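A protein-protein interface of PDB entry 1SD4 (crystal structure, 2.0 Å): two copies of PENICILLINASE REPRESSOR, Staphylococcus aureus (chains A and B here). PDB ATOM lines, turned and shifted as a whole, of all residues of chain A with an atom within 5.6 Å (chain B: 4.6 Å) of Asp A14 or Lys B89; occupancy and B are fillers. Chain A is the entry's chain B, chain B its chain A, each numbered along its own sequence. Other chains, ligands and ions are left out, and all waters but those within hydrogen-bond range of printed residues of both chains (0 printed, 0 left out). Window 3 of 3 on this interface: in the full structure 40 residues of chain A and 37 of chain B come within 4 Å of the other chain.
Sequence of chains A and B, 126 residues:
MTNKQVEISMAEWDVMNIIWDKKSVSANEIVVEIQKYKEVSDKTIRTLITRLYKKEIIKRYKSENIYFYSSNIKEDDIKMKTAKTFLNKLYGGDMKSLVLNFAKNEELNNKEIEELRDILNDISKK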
ATOM      1  N   SER A   9      13.026  10.585 -12.562  1.00  0.00           N
ATOM      2  CA  SER A   9      12.297   9.539 -11.902  1.00  0.00           C
ATOM      3  C   SER A   9      13.285   8.770 -11.024  1.00  0.00           C
ATOM      4  O   SER A   9      14.509   8.880 -11.184  1.00  0.00           O
ATOM      5  CB  SER A   9      11.734   8.595 -12.957  1.00  0.00           C
ATOM      6  OG  SER A   9      12.804   7.823 -13.484  1.00  0.00           O
ATOM      7  N   MET A  10      12.744   7.944 -10.141  1.00  0.00           N
ATOM      8  CA  MET A  10      13.531   7.124  -9.260  1.00  0.00           C
ATOM      9  C   MET A  10      14.366   6.119 -10.089  1.00  0.00           C
ATOM     10  O   MET A  10      15.528   5.867  -9.767  1.00  0.00           O
ATOM     11  CB  MET A  10      12.586   6.415  -8.294  1.00  0.00           C
ATOM     12  CG  MET A  10      12.851   6.601  -6.800  1.00  0.00           C
ATOM     13  SD  MET A  10      13.607   8.301  -6.089  1.00  0.00           S
ATOM     14  CE  MET A  10      15.330   8.213  -6.604  1.00  0.00           C
ATOM     15  N   ALA A  11      13.794   5.561 -11.158  1.00  0.00           N
ATOM     16  CA  ALA A  11      14.560   4.643 -12.022  1.00  0.00           C
ATOM     17  C   ALA A  11      15.728   5.407 -12.694  1.00  0.00           C
ATOM     18  O   ALA A  11      16.839   4.910 -12.801  1.00  0.00           O
ATOM     19  CB  ALA A  11      13.654   3.986 -13.091  1.00  0.00           C
ATOM     20  N   GLU A  12      15.470   6.610 -13.151  1.00  0.00           N
ATOM     21  CA  GLU A  12      16.525   7.416 -13.753  1.00  0.00           C
ATOM     22  C   GLU A  12      17.616   7.815 -12.728  1.00  0.00           C
ATOM     23  O   GLU A  12      18.791   7.982 -13.088  1.00  0.00           O
ATOM     24  CB  GLU A  12      15.905   8.679 -14.347  1.00  0.00           C
ATOM     25  CG  GLU A  12      15.083   8.421 -15.573  1.00  0.00           C
ATOM     26  CD  GLU A  12      14.357   9.644 -16.095  1.00  0.00           C
ATOM     27  OE1 GLU A  12      14.040  10.547 -15.337  1.00  0.00           O
ATOM     28  OE2 GLU A  12      14.073   9.675 -17.289  1.00  0.00           O
ATOM     29  N   TRP A  13      17.216   7.978 -11.468  1.00  0.00           N
ATOM     30  CA  TRP A  13      18.129   8.381 -10.427  1.00  0.00           C
ATOM     31  C   TRP A  13      19.239   7.339 -10.223  1.00  0.00           C
ATOM     32  O   TRP A  13      20.360   7.717  -9.930  1.00  0.00           O
ATOM     33  CB  TRP A  13      17.395   8.615  -9.092  1.00  0.00           C
ATOM     34  CG  TRP A  13      18.102   9.644  -8.249  1.00  0.00           C
ATOM     35  CD1 TRP A  13      19.192   9.438  -7.404  1.00  0.00           C
ATOM     36  CD2 TRP A  13      17.800  11.048  -8.176  1.00  0.00           C
ATOM     37  NE1 TRP A  13      19.571  10.640  -6.845  1.00  0.00           N
ATOM     38  CE2 TRP A  13      18.744  11.640  -7.293  1.00  0.00           C
ATOM     39  CE3 TRP A  13      16.819  11.874  -8.773  1.00  0.00           C
ATOM     40  CZ2 TRP A  13      18.744  13.021  -7.000  1.00  0.00           C
ATOM     41  CZ3 TRP A  13      16.822  13.238  -8.482  1.00  0.00           C
ATOM     42  CH2 TRP A  13      17.770  13.794  -7.593  1.00  0.00           C
ATOM     43  N   ASP A  14      18.934   6.051 -10.390  1.00  0.00           N
ATOM     44  CA  ASP A  14      19.974   5.042 -10.310  1.00  0.00           C
ATOM     45  C   ASP A  14      21.062   5.321 -11.327  1.00  0.00           C
ATOM     46  O   ASP A  14      22.242   5.144 -11.034  1.00  0.00           O
ATOM     47  CB  ASP A  14      19.435   3.645 -10.605  1.00  0.00           C
ATOM     48  CG  ASP A  14      18.413   3.173  -9.580  1.00  0.00           C
ATOM     49  OD1 ASP A  14      18.480   3.594  -8.419  1.00  0.00           O
ATOM     50  OD2 ASP A  14      17.495   2.388  -9.876  1.00  0.00           O
ATOM     51  N   VAL A  15      20.680   5.702 -12.543  1.00  0.00           N
ATOM     52  CA  VAL A  15      21.679   6.042 -13.561  1.00  0.00           C
ATOM     53  C   VAL A  15      22.492   7.296 -13.114  1.00  0.00           C
ATOM     54  O   VAL A  15      23.713   7.318 -13.174  1.00  0.00           O
ATOM     55  CB  VAL A  15      21.007   6.270 -14.954  1.00  0.00           C
ATOM     56  CG1 VAL A  15      21.976   6.849 -15.935  1.00  0.00           C
ATOM     57  CG2 VAL A  15      20.448   4.956 -15.542  1.00  0.00           C
ATOM     58  N   MET A  16      21.796   8.337 -12.699  1.00  0.00           N
ATOM     59  CA  MET A  16      22.458   9.561 -12.249  1.00  0.00           C
ATOM     60  C   MET A  16      23.443   9.312 -11.120  1.00  0.00           C
ATOM     61  O   MET A  16      24.512   9.899 -11.107  1.00  0.00           O
ATOM     62  CB  MET A  16      21.463  10.619 -11.852  1.00  0.00           C
ATOM     63  CG  MET A  16      20.548  11.086 -13.009  1.00  0.00           C
ATOM     64  SD  MET A  16      21.547  11.640 -14.634  1.00  0.00           S
ATOM     65  CE  MET A  16      22.845  12.894 -13.744  1.00  0.00           C
ATOM     66  N   ASN A  17      23.113   8.411 -10.205  1.00  0.00           N
ATOM     67  CA  ASN A  17      24.048   8.102  -9.135  1.00  0.00           C
ATOM     68  C   ASN A  17      25.405   7.630  -9.693  1.00  0.00           C
ATOM     69  O   ASN A  17      26.472   7.987  -9.167  1.00  0.00           O
ATOM     70  CB  ASN A  17      23.452   7.099  -8.151  1.00  0.00           C
ATOM     71  CG  ASN A  17      22.590   7.761  -7.087  1.00  0.00           C
ATOM     72  OD1 ASN A  17      22.630   8.981  -6.892  1.00  0.00           O
ATOM     73  ND2 ASN A  17      21.776   6.952  -6.394  1.00  0.00           N
ATOM     74  N   ILE A  18      25.381   6.886 -10.786  1.00  0.00           N
ATOM     75  CA  ILE A  18      26.621   6.426 -11.401  1.00  0.00           C
ATOM     76  C   ILE A  18      27.323   7.538 -12.215  1.00  0.00           C
ATOM     77  O   ILE A  18      28.554   7.673 -12.172  1.00  0.00           O
ATOM     78  CB  ILE A  18      26.361   5.202 -12.263  1.00  0.00           C
ATOM     79  CG1 ILE A  18      25.858   4.029 -11.401  1.00  0.00           C
ATOM     80  CG2 ILE A  18      27.603   4.825 -13.085  1.00  0.00           C
ATOM     81  CD1 ILE A  18      24.920   3.169 -12.199  1.00  0.00           C
ATOM     82  N   ILE A  34      24.545  -0.808 -12.533  1.00  0.00           N
ATOM     83  CA  ILE A  34      23.155  -0.974 -12.091  1.00  0.00           C
ATOM     84  C   ILE A  34      22.746  -2.464 -11.928  1.00  0.00           C
ATOM     85  O   ILE A  34      21.973  -2.833 -11.041  1.00  0.00           O
ATOM     86  CB  ILE A  34      22.203  -0.316 -13.086  1.00  0.00           C
ATOM     87  CG1 ILE A  34      22.274   1.224 -12.916  1.00  0.00           C
ATOM     88  CG2 ILE A  34      20.726  -0.852 -12.880  1.00  0.00           C
ATOM     89  CD1 ILE A  34      21.752   1.986 -14.072  1.00  0.00           C
ATOM     90  N   TYR A  37      22.864  -4.601  -8.696  1.00  0.00           N
ATOM     91  CA  TYR A  37      21.881  -4.582  -7.600  1.00  0.00           C
ATOM     92  C   TYR A  37      20.429  -4.491  -8.040  1.00  0.00           C
ATOM     93  O   TYR A  37      19.508  -4.492  -7.209  1.00  0.00           O
ATOM     94  CB  TYR A  37      22.220  -3.486  -6.567  1.00  0.00           C
ATOM     95  CG  TYR A  37      22.267  -2.114  -7.181  1.00  0.00           C
ATOM     96  CD1 TYR A  37      23.451  -1.637  -7.739  1.00  0.00           C
ATOM     97  CD2 TYR A  37      21.120  -1.305  -7.239  1.00  0.00           C
ATOM     98  CE1 TYR A  37      23.504  -0.393  -8.331  1.00  0.00           C
ATOM     99  CE2 TYR A  37      21.165  -0.046  -7.817  1.00  0.00           C
ATOM    100  CZ  TYR A  37      22.373   0.397  -8.360  1.00  0.00           C
ATOM    101  OH  TYR A  37      22.479   1.616  -8.951  1.00  0.00           O
ATOM    102  N   LYS A  38      20.205  -4.445  -9.350  1.00  0.00           N
ATOM    103  CA  LYS A  38      18.850  -4.437  -9.882  1.00  0.00           C
ATOM    104  C   LYS A  38      18.732  -5.422 -11.045  1.00  0.00           C
ATOM    105  O   LYS A  38      19.695  -5.614 -11.765  1.00  0.00           O
ATOM    106  CB  LYS A  38      18.548  -3.019 -10.364  1.00  0.00           C
ATOM    107  CG  LYS A  38      17.115  -2.585 -10.190  1.00  0.00           C
ATOM    108  CD  LYS A  38      17.010  -1.044 -10.229  1.00  0.00           C
ATOM    109  CE  LYS A  38      15.593  -0.624  -9.925  1.00  0.00           C
ATOM    110  NZ  LYS A  38      14.601  -1.414 -10.711  1.00  0.00           N
ATOM    111  N   LYS A  79      18.278  17.455  -6.637  1.00  0.00           N
ATOM    112  CA  LYS A  79      17.878  16.691  -5.456  1.00  0.00           C
ATOM    113  C   LYS A  79      16.860  17.462  -4.630  1.00  0.00           C
ATOM    114  O   LYS A  79      15.839  16.937  -4.238  1.00  0.00           O
ATOM    115  CB  LYS A  79      19.076  16.335  -4.593  1.00  0.00           C
ATOM    116  CG  LYS A  79      18.678  15.403  -3.419  1.00  0.00           C
ATOM    117  CD  LYS A  79      19.777  15.266  -2.364  1.00  0.00           C
ATOM    118  CE  LYS A  79      21.086  14.804  -2.997  1.00  0.00           C
ATOM    119  NZ  LYS A  79      21.144  13.349  -3.202  1.00  0.00           N
ATOM    120  N   THR B  85      11.696   4.331  -0.514  1.00  0.00           N
ATOM    121  CA  THR B  85      12.595   4.222  -1.667  1.00  0.00           C
ATOM    122  C   THR B  85      13.251   5.574  -1.951  1.00  0.00           C
ATOM    123  O   THR B  85      14.450   5.654  -2.269  1.00  0.00           O
ATOM    124  CB  THR B  85      11.789   3.778  -2.900  1.00  0.00           C
ATOM    125  OG1 THR B  85      11.355   2.432  -2.689  1.00  0.00           O
ATOM    126  CG2 THR B  85      12.674   3.747  -4.181  1.00  0.00           C
ATOM    127  N   PHE B  86      12.468   6.628  -1.830  1.00  0.00           N
ATOM    128  CA  PHE B  86      12.957   8.003  -2.012  1.00  0.00           C
ATOM    129  C   PHE B  86      14.091   8.357  -1.023  1.00  0.00           C
ATOM    130  O   PHE B  86      15.171   8.796  -1.422  1.00  0.00           O
ATOM    131  CB  PHE B  86      11.799   8.971  -1.786  1.00  0.00           C
ATOM    132  CG  PHE B  86      12.191  10.414  -1.897  1.00  0.00           C
ATOM    133  CD1 PHE B  86      12.440  10.971  -3.150  1.00  0.00           C
ATOM    134  CD2 PHE B  86      12.304  11.217  -0.760  1.00  0.00           C
ATOM    135  CE1 PHE B  86      12.824  12.309  -3.276  1.00  0.00           C
ATOM    136  CE2 PHE B  86      12.702  12.591  -0.864  1.00  0.00           C
ATOM    137  CZ  PHE B  86      12.947  13.120  -2.126  1.00  0.00           C
ATOM    138  N   LEU B  87      13.811   8.160   0.259  1.00  0.00           N
ATOM    139  CA  LEU B  87      14.769   8.453   1.334  1.00  0.00           C
ATOM    140  C   LEU B  87      16.046   7.648   1.172  1.00  0.00           C
ATOM    141  O   LEU B  87      17.170   8.186   1.268  1.00  0.00           O
ATOM    142  CB  LEU B  87      14.101   8.267   2.719  1.00  0.00           C
ATOM    143  CG  LEU B  87      14.799   8.920   3.929  1.00  0.00           C
ATOM    144  CD1 LEU B  87      14.756  10.441   3.896  1.00  0.00           C
ATOM    145  CD2 LEU B  87      14.209   8.360   5.222  1.00  0.00           C
ATOM    146  N   ASN B  88      15.887   6.371   0.851  1.00  0.00           N
ATOM    147  CA  ASN B  88      17.048   5.508   0.620  1.00  0.00           C
ATOM    148  C   ASN B  88      17.959   6.005  -0.507  1.00  0.00           C
ATOM    149  O   ASN B  88      19.191   5.998  -0.376  1.00  0.00           O
ATOM    150  CB  ASN B  88      16.625   4.053   0.349  1.00  0.00           C
ATOM    151  CG  ASN B  88      16.099   3.364   1.604  1.00  0.00           C
ATOM    152  OD1 ASN B  88      16.327   3.839   2.731  1.00  0.00           O
ATOM    153  ND2 ASN B  88      15.376   2.249   1.423  1.00  0.00           N
ATOM    154  N   LYS B  89      17.357   6.396  -1.615  1.00  0.00           N
ATOM    155  CA  LYS B  89      18.138   6.758  -2.788  1.00  0.00           C
ATOM    156  C   LYS B  89      18.757   8.137  -2.694  1.00  0.00           C
ATOM    157  O   LYS B  89      19.876   8.330  -3.133  1.00  0.00           O
ATOM    158  CB  LYS B  89      17.302   6.670  -4.082  1.00  0.00           C
ATOM    159  CG  LYS B  89      18.116   5.997  -5.209  1.00  0.00           C
ATOM    160  CD  LYS B  89      17.379   5.831  -6.551  1.00  0.00           C
ATOM    161  CE  LYS B  89      16.114   4.978  -6.457  1.00  0.00           C
ATOM    162  NZ  LYS B  89      16.426   3.527  -6.415  1.00  0.00           N
ATOM    163  N   LEU B  90      18.004   9.108  -2.191  1.00  0.00           N
ATOM    164  CA  LEU B  90      18.479  10.486  -2.193  1.00  0.00           C
ATOM    165  C   LEU B  90      19.163  10.888  -0.908  1.00  0.00           C
ATOM    166  O   LEU B  90      19.940  11.809  -0.914  1.00  0.00           O
ATOM    167  CB  LEU B  90      17.328  11.450  -2.484  1.00  0.00           C
ATOM    168  CG  LEU B  90      17.092  11.643  -3.994  1.00  0.00           C
ATOM    169  CD1 LEU B  90      16.812  10.291  -4.719  1.00  0.00           C
ATOM    170  CD2 LEU B  90      15.918  12.549  -4.159  1.00  0.00           C
ATOM    171  N   TYR B  91      18.829  10.236   0.201  1.00  0.00           N
ATOM    172  CA  TYR B  91      19.310  10.696   1.511  1.00  0.00           C
ATOM    173  C   TYR B  91      19.914   9.569   2.328  1.00  0.00           C
ATOM    174  O   TYR B  91      19.884   9.628   3.555  1.00  0.00           O
ATOM    175  CB  TYR B  91      18.204  11.430   2.294  1.00  0.00           C
ATOM    176  CG  TYR B  91      17.811  12.733   1.604  1.00  0.00           C
ATOM    177  CD1 TYR B  91      18.615  13.882   1.707  1.00  0.00           C
ATOM    178  CD2 TYR B  91      16.677  12.798   0.813  1.00  0.00           C
ATOM    179  CE1 TYR B  91      18.283  15.077   1.040  1.00  0.00           C
ATOM    180  CE2 TYR B  91      16.319  13.979   0.143  1.00  0.00           C
ATOM    181  CZ  TYR B  91      17.140  15.117   0.259  1.00  0.00           C
ATOM    182  OH  TYR B  91      16.795  16.289  -0.384  1.00  0.00           O
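Hydrophobic or aromatic side chains of chain A within 4 Å of the printed part of chain B: Met A10 and Trp A13.
NZ of Lys B89 is in salt-bridge range of OD1 of Asp A14, at 2.9 Å.
O of Leu B90 lies within hydrogen-bond range of NZ of Lys A79, at 3.0 Å.
Of the printed residues of chain B, Trp A13 touches Lys B89 (3.8 Å) and Leu B90 (3.5 Å).
Asp A14 touches just one residue of chain B: Lys B89 (2.9 Å).
Met A16 touches none of the printed residues of chain B.
Ile A34 touches none of the printed residues of chain B.
Of the printed residues of chain B, Lys A79 touches Leu B90 and Tyr B91.
Of the printed residues of chain A, Lys B89 touches Met A10, Trp A13, Asp A14 and Asn A17.
The nearest residue of chain A that does not touch Lys B89 is Lys A79 (5.2 Å).
The nearest printed residue of chain B that does not touch Met A10 is Phe B86 (4.1 Å).
CG2 of Thr B85 touches CG of Met A10, at 3.9 Å.
Lys B89 touches Met A10.
CD1 of Leu B90 touches CE of Met A10, at 3.2 Å.
CB of Trp A13 touches CD of Lys B89, at 3.8 Å.
Trp A13 touches Leu B90 (CE2 to CD1, 3.5 Å).
Asn A17 touches Lys B89.
Lys A79 touches Tyr B91.
The indole nitrogen (NE1) of Trp A13 is in hydrogen-bond range of the side-chain amide oxygen (OD1) of Asn A17 (3.5 Å).
No position is printed for both chains.
Of the 9 pairs that touch across the chains among the printed residues, none has its exchanged pair printed and touching as well.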
